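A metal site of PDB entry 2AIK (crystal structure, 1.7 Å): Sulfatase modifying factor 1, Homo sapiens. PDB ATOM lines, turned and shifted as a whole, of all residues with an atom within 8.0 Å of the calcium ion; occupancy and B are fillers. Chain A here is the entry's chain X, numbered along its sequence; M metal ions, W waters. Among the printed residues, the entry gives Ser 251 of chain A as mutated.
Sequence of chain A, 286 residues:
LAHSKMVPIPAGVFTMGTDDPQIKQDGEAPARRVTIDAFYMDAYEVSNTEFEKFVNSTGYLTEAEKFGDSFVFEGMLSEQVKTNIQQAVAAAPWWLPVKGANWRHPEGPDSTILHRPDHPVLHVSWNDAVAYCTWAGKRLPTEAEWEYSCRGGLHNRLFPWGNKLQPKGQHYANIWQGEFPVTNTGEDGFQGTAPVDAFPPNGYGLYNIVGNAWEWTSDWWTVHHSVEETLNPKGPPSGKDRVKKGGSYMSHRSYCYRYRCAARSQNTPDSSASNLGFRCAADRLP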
ATOM      1  N   HIS A 171      14.161  -6.841  23.741  1.00  0.00           N
ATOM      2  CA  HIS A 171      14.684  -8.187  23.861  1.00  0.00           C
ATOM      3  C   HIS A 171      15.404  -8.542  22.573  1.00  0.00           C
ATOM      4  O   HIS A 171      14.851  -8.323  21.474  1.00  0.00           O
ATOM      5  CB  HIS A 171      13.548  -9.180  24.187  1.00  0.00           C
ATOM      6  CG  HIS A 171      13.155  -9.166  25.624  1.00  0.00           C
ATOM      7  ND1 HIS A 171      13.935  -9.734  26.601  1.00  0.00           N
ATOM      8  CD2 HIS A 171      12.114  -8.579  26.259  1.00  0.00           C
ATOM      9  CE1 HIS A 171      13.380  -9.529  27.778  1.00  0.00           C
ATOM     10  NE2 HIS A 171      12.291  -8.801  27.601  1.00  0.00           N
ATOM     11  N   ALA A 173      17.148 -11.777  22.273  1.00  0.00           N
ATOM     12  CA  ALA A 173      17.303 -13.222  22.243  1.00  0.00           C
ATOM     13  C   ALA A 173      16.225 -13.879  23.095  1.00  0.00           C
ATOM     14  O   ALA A 173      15.673 -13.254  24.028  1.00  0.00           O
ATOM     15  CB  ALA A 173      18.654 -13.628  22.766  1.00  0.00           C
ATOM     16  N   ASN A 174      15.962 -15.143  22.791  1.00  0.00           N
ATOM     17  CA  ASN A 174      14.981 -15.945  23.496  1.00  0.00           C
ATOM     18  C   ASN A 174      15.678 -16.739  24.619  1.00  0.00           C
ATOM     19  O   ASN A 174      16.300 -17.768  24.378  1.00  0.00           O
ATOM     20  CB  ASN A 174      14.238 -16.881  22.558  1.00  0.00           C
ATOM     21  CG  ASN A 174      13.225 -17.730  23.276  1.00  0.00           C
ATOM     22  OD1 ASN A 174      12.818 -17.384  24.412  1.00  0.00           O
ATOM     23  ND2 ASN A 174      12.797 -18.836  22.663  1.00  0.00           N
ATOM     24  N   ILE A 175      15.576 -16.215  25.838  1.00  0.00           N
ATOM     25  CA  ILE A 175      16.102 -16.890  27.040  1.00  0.00           C
ATOM     26  C   ILE A 175      14.959 -16.933  28.072  1.00  0.00           C
ATOM     27  O   ILE A 175      13.811 -16.701  27.725  1.00  0.00           O
ATOM     28  CB  ILE A 175      17.421 -16.243  27.560  1.00  0.00           C
ATOM     29  CG1 ILE A 175      17.253 -14.744  27.906  1.00  0.00           C
ATOM     30  CG2 ILE A 175      18.479 -16.425  26.514  1.00  0.00           C
ATOM     31  CD1 ILE A 175      18.410 -14.187  28.700  1.00  0.00           C
ATOM     32  N   TRP A 176      15.294 -17.177  29.338  1.00  0.00           N
ATOM     33  CA  TRP A 176      14.316 -17.262  30.403  1.00  0.00           C
ATOM     34  C   TRP A 176      14.131 -15.894  31.047  1.00  0.00           C
ATOM     35  O   TRP A 176      15.100 -15.154  31.246  1.00  0.00           O
ATOM     36  CB  TRP A 176      14.813 -18.251  31.429  1.00  0.00           C
ATOM     37  CG  TRP A 176      13.865 -18.628  32.521  1.00  0.00           C
ATOM     38  CD1 TRP A 176      13.592 -17.947  33.654  1.00  0.00           C
ATOM     39  CD2 TRP A 176      13.135 -19.841  32.585  1.00  0.00           C
ATOM     40  NE1 TRP A 176      12.709 -18.663  34.453  1.00  0.00           N
ATOM     41  CE2 TRP A 176      12.417 -19.840  33.808  1.00  0.00           C
ATOM     42  CE3 TRP A 176      12.997 -20.936  31.725  1.00  0.00           C
ATOM     43  CZ2 TRP A 176      11.563 -20.888  34.171  1.00  0.00           C
ATOM     44  CZ3 TRP A 176      12.172 -21.989  32.088  1.00  0.00           C
ATOM     45  CH2 TRP A 176      11.467 -21.955  33.297  1.00  0.00           C
ATOM     46  N   GLN A 177      12.880 -15.534  31.351  1.00  0.00           N
ATOM     47  CA  GLN A 177      12.630 -14.453  32.311  1.00  0.00           C
ATOM     48  C   GLN A 177      11.809 -15.024  33.433  1.00  0.00           C
ATOM     49  O   GLN A 177      10.897 -15.784  33.205  1.00  0.00           O
ATOM     50  CB  GLN A 177      11.890 -13.262  31.713  1.00  0.00           C
ATOM     51  CG  GLN A 177      12.679 -12.517  30.664  1.00  0.00           C
ATOM     52  CD  GLN A 177      12.512 -13.153  29.313  1.00  0.00           C
ATOM     53  OE1 GLN A 177      11.405 -13.538  28.942  1.00  0.00           O
ATOM     54  NE2 GLN A 177      13.623 -13.273  28.569  1.00  0.00           N
ATOM     55  N   ASN A 184       8.602 -19.180  34.156  1.00  0.00           N
ATOM     56  CA  ASN A 184       9.045 -18.450  32.978  1.00  0.00           C
ATOM     57  C   ASN A 184       7.923 -17.511  32.571  1.00  0.00           C
ATOM     58  O   ASN A 184       6.831 -17.927  32.178  1.00  0.00           O
ATOM     59  CB  ASN A 184       9.372 -19.426  31.863  1.00  0.00           C
ATOM     60  CG  ASN A 184      10.006 -18.767  30.674  1.00  0.00           C
ATOM     61  OD1 ASN A 184       9.985 -17.562  30.535  1.00  0.00           O
ATOM     62  ND2 ASN A 184      10.598 -19.576  29.808  1.00  0.00           N
ATOM     63  N   THR A 185       8.185 -16.211  32.669  1.00  0.00           N
ATOM     64  CA  THR A 185       7.126 -15.244  32.436  1.00  0.00           C
ATOM     65  C   THR A 185       6.784 -15.071  30.948  1.00  0.00           C
ATOM     66  O   THR A 185       5.721 -14.565  30.633  1.00  0.00           O
ATOM     67  CB  THR A 185       7.501 -13.860  32.997  1.00  0.00           C
ATOM     68  OG1 THR A 185       8.575 -13.337  32.227  1.00  0.00           O
ATOM     69  CG2 THR A 185       7.889 -13.948  34.446  1.00  0.00           C
ATOM     70  N   GLY A 186       7.686 -15.471  30.046  1.00  0.00           N
ATOM     71  CA  GLY A 186       7.467 -15.297  28.602  1.00  0.00           C
ATOM     72  C   GLY A 186       7.485 -13.837  28.200  1.00  0.00           C
ATOM     73  O   GLY A 186       6.899 -13.451  27.185  1.00  0.00           O
ATOM     74  N   GLU A 187       8.197 -13.035  28.984  1.00  0.00           N
ATOM     75  CA  GLU A 187       8.323 -11.602  28.699  1.00  0.00           C
ATOM     76  C   GLU A 187       8.875 -11.321  27.303  1.00  0.00           C
ATOM     77  O   GLU A 187       8.430 -10.382  26.624  1.00  0.00           O
ATOM     78  CB  GLU A 187       9.214 -10.966  29.749  1.00  0.00           C
ATOM     79  CG  GLU A 187       9.424  -9.486  29.584  1.00  0.00           C
ATOM     80  CD  GLU A 187      10.516  -8.971  30.502  1.00  0.00           C
ATOM     81  OE1 GLU A 187      10.731  -9.551  31.596  1.00  0.00           O
ATOM     82  OE2 GLU A 187      11.172  -8.008  30.091  1.00  0.00           O
ATOM     83  N   ASP A 188       9.829 -12.146  26.856  1.00  0.00           N
ATOM     84  CA  ASP A 188      10.455 -11.931  25.553  1.00  0.00           C
ATOM     85  C   ASP A 188       9.589 -12.430  24.377  1.00  0.00           C
ATOM     86  O   ASP A 188       9.971 -12.285  23.206  1.00  0.00           O
ATOM     87  CB  ASP A 188      11.850 -12.521  25.511  1.00  0.00           C
ATOM     88  CG  ASP A 188      11.873 -14.027  25.685  1.00  0.00           C
ATOM     89  OD1 ASP A 188      10.848 -14.721  25.440  1.00  0.00           O
ATOM     90  OD2 ASP A 188      12.969 -14.539  26.024  1.00  0.00           O
ATOM     91  N   GLY A 189       8.423 -12.998  24.706  1.00  0.00           N
ATOM     92  CA  GLY A 189       7.446 -13.406  23.711  1.00  0.00           C
ATOM     93  C   GLY A 189       7.389 -14.892  23.454  1.00  0.00           C
ATOM     94  O   GLY A 189       6.551 -15.336  22.654  1.00  0.00           O
ATOM     95  N   PHE A 190       8.293 -15.675  24.074  1.00  0.00           N
ATOM     96  CA  PHE A 190       8.368 -17.132  23.878  1.00  0.00           C
ATOM     97  C   PHE A 190       8.738 -17.825  25.167  1.00  0.00           C
ATOM     98  O   PHE A 190       9.749 -17.524  25.757  1.00  0.00           O
ATOM     99  CB  PHE A 190       9.406 -17.455  22.788  1.00  0.00           C
ATOM    100  CG  PHE A 190       9.101 -16.776  21.505  1.00  0.00           C
ATOM    101  CD1 PHE A 190       8.196 -17.359  20.593  1.00  0.00           C
ATOM    102  CD2 PHE A 190       9.631 -15.524  21.218  1.00  0.00           C
ATOM    103  CE1 PHE A 190       7.848 -16.708  19.419  1.00  0.00           C
ATOM    104  CE2 PHE A 190       9.305 -14.883  20.049  1.00  0.00           C
ATOM    105  CZ  PHE A 190       8.399 -15.472  19.150  1.00  0.00           C
ATOM    106  N   GLN A 191       7.891 -18.746  25.622  1.00  0.00           N
ATOM    107  CA  GLN A 191       8.227 -19.604  26.750  1.00  0.00           C
ATOM    108  C   GLN A 191       9.158 -20.736  26.316  1.00  0.00           C
ATOM    109  O   GLN A 191      10.176 -20.979  26.949  1.00  0.00           O
ATOM    110  CB  GLN A 191       6.969 -20.128  27.406  1.00  0.00           C
ATOM    111  CG  GLN A 191       6.368 -19.014  28.230  1.00  0.00           C
ATOM    112  CD  GLN A 191       5.066 -19.336  28.828  1.00  0.00           C
ATOM    113  OE1 GLN A 191       4.187 -19.910  28.156  1.00  0.00           O
ATOM    114  NE2 GLN A 191       4.870 -18.916  30.080  1.00  0.00           N
ATOM    115  N   GLY A 192       8.781 -21.447  25.258  1.00  0.00           N
ATOM    116  CA  GLY A 192       9.656 -22.461  24.680  1.00  0.00           C
ATOM    117  C   GLY A 192      10.474 -21.833  23.580  1.00  0.00           C
ATOM    118  O   GLY A 192      10.896 -20.674  23.683  1.00  0.00           O
ATOM    119  N   THR A 193      10.683 -22.584  22.492  1.00  0.00           N
ATOM    120  CA  THR A 193      11.437 -22.045  21.364  1.00  0.00           C
ATOM    121  C   THR A 193      10.630 -20.995  20.613  1.00  0.00           C
ATOM    122  O   THR A 193       9.381 -20.837  20.778  1.00  0.00           O
ATOM    123  CB  THR A 193      11.815 -23.185  20.368  1.00  0.00           C
ATOM    124  OG1 THR A 193      10.634 -23.864  19.965  1.00  0.00           O
ATOM    125  CG2 THR A 193      12.758 -24.162  21.026  1.00  0.00           C
ATOM    126  N   ALA A 194      11.368 -20.221  19.822  1.00  0.00           N
ATOM    127  CA  ALA A 194      10.826 -19.269  18.877  1.00  0.00           C
ATOM    128  C   ALA A 194      11.151 -19.702  17.454  1.00  0.00           C
ATOM    129  O   ALA A 194      12.083 -20.481  17.245  1.00  0.00           O
ATOM    130  CB  ALA A 194      11.442 -17.856  19.115  1.00  0.00           C
ATOM    131  N   PHE A 199      13.733 -12.426  16.459  1.00  0.00           N
ATOM    132  CA  PHE A 199      14.700 -11.521  17.097  1.00  0.00           C
ATOM    133  C   PHE A 199      15.655 -10.888  16.085  1.00  0.00           C
ATOM    134  O   PHE A 199      15.712 -11.310  14.939  1.00  0.00           O
ATOM    135  CB  PHE A 199      15.417 -12.190  18.272  1.00  0.00           C
ATOM    136  CG  PHE A 199      14.471 -12.558  19.392  1.00  0.00           C
ATOM    137  CD1 PHE A 199      14.002 -11.556  20.242  1.00  0.00           C
ATOM    138  CD2 PHE A 199      13.981 -13.830  19.488  1.00  0.00           C
ATOM    139  CE1 PHE A 199      13.064 -11.842  21.206  1.00  0.00           C
ATOM    140  CE2 PHE A 199      13.044 -14.147  20.467  1.00  0.00           C
ATOM    141  CZ  PHE A 199      12.587 -13.135  21.324  1.00  0.00           C
ATOM    142  N   ASN A 212      17.424 -19.494  22.336  1.00  0.00           N
ATOM    143  CA  ASN A 212      16.556 -20.352  21.532  1.00  0.00           C
ATOM    144  C   ASN A 212      16.975 -21.810  21.720  1.00  0.00           C
ATOM    145  O   ASN A 212      16.630 -22.405  22.761  1.00  0.00           O
ATOM    146  CB  ASN A 212      16.440 -19.875  20.072  1.00  0.00           C
ATOM    147  CG  ASN A 212      15.032 -20.106  19.482  1.00  0.00           C
ATOM    148  OD1 ASN A 212      14.030 -20.021  20.202  1.00  0.00           O
ATOM    149  ND2 ASN A 212      14.956 -20.346  18.171  1.00  0.00           N
ATOM    150  N   SER A 248      20.175 -21.255  25.478  1.00  0.00           N
ATOM    151  CA  SER A 248      18.861 -21.645  25.013  1.00  0.00           C
ATOM    152  C   SER A 248      17.761 -20.822  25.654  1.00  0.00           C
ATOM    153  O   SER A 248      18.000 -19.973  26.522  1.00  0.00           O
ATOM    154  CB  SER A 248      18.590 -23.127  25.339  1.00  0.00           C
ATOM    155  OG  SER A 248      18.191 -23.324  26.697  1.00  0.00           O
ATOM    156  N   TYR A 249      16.544 -21.106  25.222  1.00  0.00           N
ATOM    157  CA  TYR A 249      15.354 -20.515  25.837  1.00  0.00           C
ATOM    158  C   TYR A 249      15.227 -20.732  27.362  1.00  0.00           C
ATOM    159  O   TYR A 249      14.414 -20.066  28.043  1.00  0.00           O
ATOM    160  CB  TYR A 249      14.116 -21.032  25.112  1.00  0.00           C
ATOM    161  CG  TYR A 249      13.706 -22.463  25.372  1.00  0.00           C
ATOM    162  CD1 TYR A 249      13.999 -23.475  24.452  1.00  0.00           C
ATOM    163  CD2 TYR A 249      12.964 -22.790  26.493  1.00  0.00           C
ATOM    164  CE1 TYR A 249      13.565 -24.796  24.688  1.00  0.00           C
ATOM    165  CE2 TYR A 249      12.553 -24.075  26.734  1.00  0.00           C
ATOM    166  CZ  TYR A 249      12.833 -25.072  25.844  1.00  0.00           C
ATOM    167  OH  TYR A 249      12.396 -26.369  26.076  1.00  0.00           O
ATOM    168  N   MET A 250      16.012 -21.661  27.886  1.00  0.00           N
ATOM    169  CA  MET A 250      16.007 -21.952  29.335  1.00  0.00           C
ATOM    170  C   MET A 250      17.024 -21.147  30.101  1.00  0.00           C
ATOM    171  O   MET A 250      17.036 -21.139  31.349  1.00  0.00           O
ATOM    172  CB  MET A 250      16.285 -23.437  29.568  1.00  0.00           C
ATOM    173  CG  MET A 250      15.170 -24.376  29.210  1.00  0.00           C
ATOM    174  SD  MET A 250      15.721 -26.120  29.228  1.00  0.00           S
ATOM    175  CE  MET A 250      15.884 -26.368  30.997  1.00  0.00           C
ATOM    176  N   SER A 251      17.969 -20.517  29.384  1.00  0.00           N
ATOM    177  CA  SER A 251      19.114 -19.931  30.047  1.00  0.00           C
ATOM    178  C   SER A 251      18.725 -18.703  30.863  1.00  0.00           C
ATOM    179  O   SER A 251      17.843 -17.948  30.487  1.00  0.00           O
ATOM    180  CB  SER A 251      20.231 -19.579  29.047  1.00  0.00           C
ATOM    181  OG  SER A 251      20.706 -20.695  28.290  1.00  0.00           O
HETATM  182 CA    CA M   1      11.891 -16.736  26.388  1.00  0.00          CA
HETATM  183  O   HOH W   1      10.770 -16.126  28.342  1.00  0.00           O
HETATM  184  O   HOH W   2      12.073 -18.981  27.254  1.00  0.00           O
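The backbone carbonyl oxygen (O) of Asn 174 lies within hydrogen-bond range of the backbone NH (N) of Asn 212, 2.9 Å away. O of Asn 174 lies close to N of Tyr 249 (3.5 Å). The side-chain amide oxygen (OE1) of Gln 177 sits at hydrogen-bond distance from the backbone NH (N) of Asp 188. The side-chain amide nitrogen of Asn 174 sits close to the backbone NH of Ala 194. ND2 of Asn 174 sits at hydrogen-bond distance from O of Gly 192 (2.8 Å).
The calcium ion is bound by OD1 of Asn 174 (2.3 Å), water W1 (2.3 Å), O of Ile 175 (2.3 Å), O of Phe 190 (2.4 Å), water W2 (2.4 Å), OD1 of Asp 188 (2.5 Å) and OD2 of Asp 188 (2.5 Å). The calcium ion has seven donor atoms within binding distance.
Within 4 Å of the calcium ion: Asn 174, Ile 175, Asp 188 and Phe 190.
Water W1 lies within hydrogen-bond range of the side-chain amide oxygen (OE1) of Gln 177 (2.7 Å) and the side-chain amide oxygen (OD1) of Asn 184 (2.7 Å). Water W2 lies within hydrogen-bond range of O of Tyr 249 (2.7 Å), O of Gln 191 (2.8 Å) and ND2 of Asn 184 (3.0 Å).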
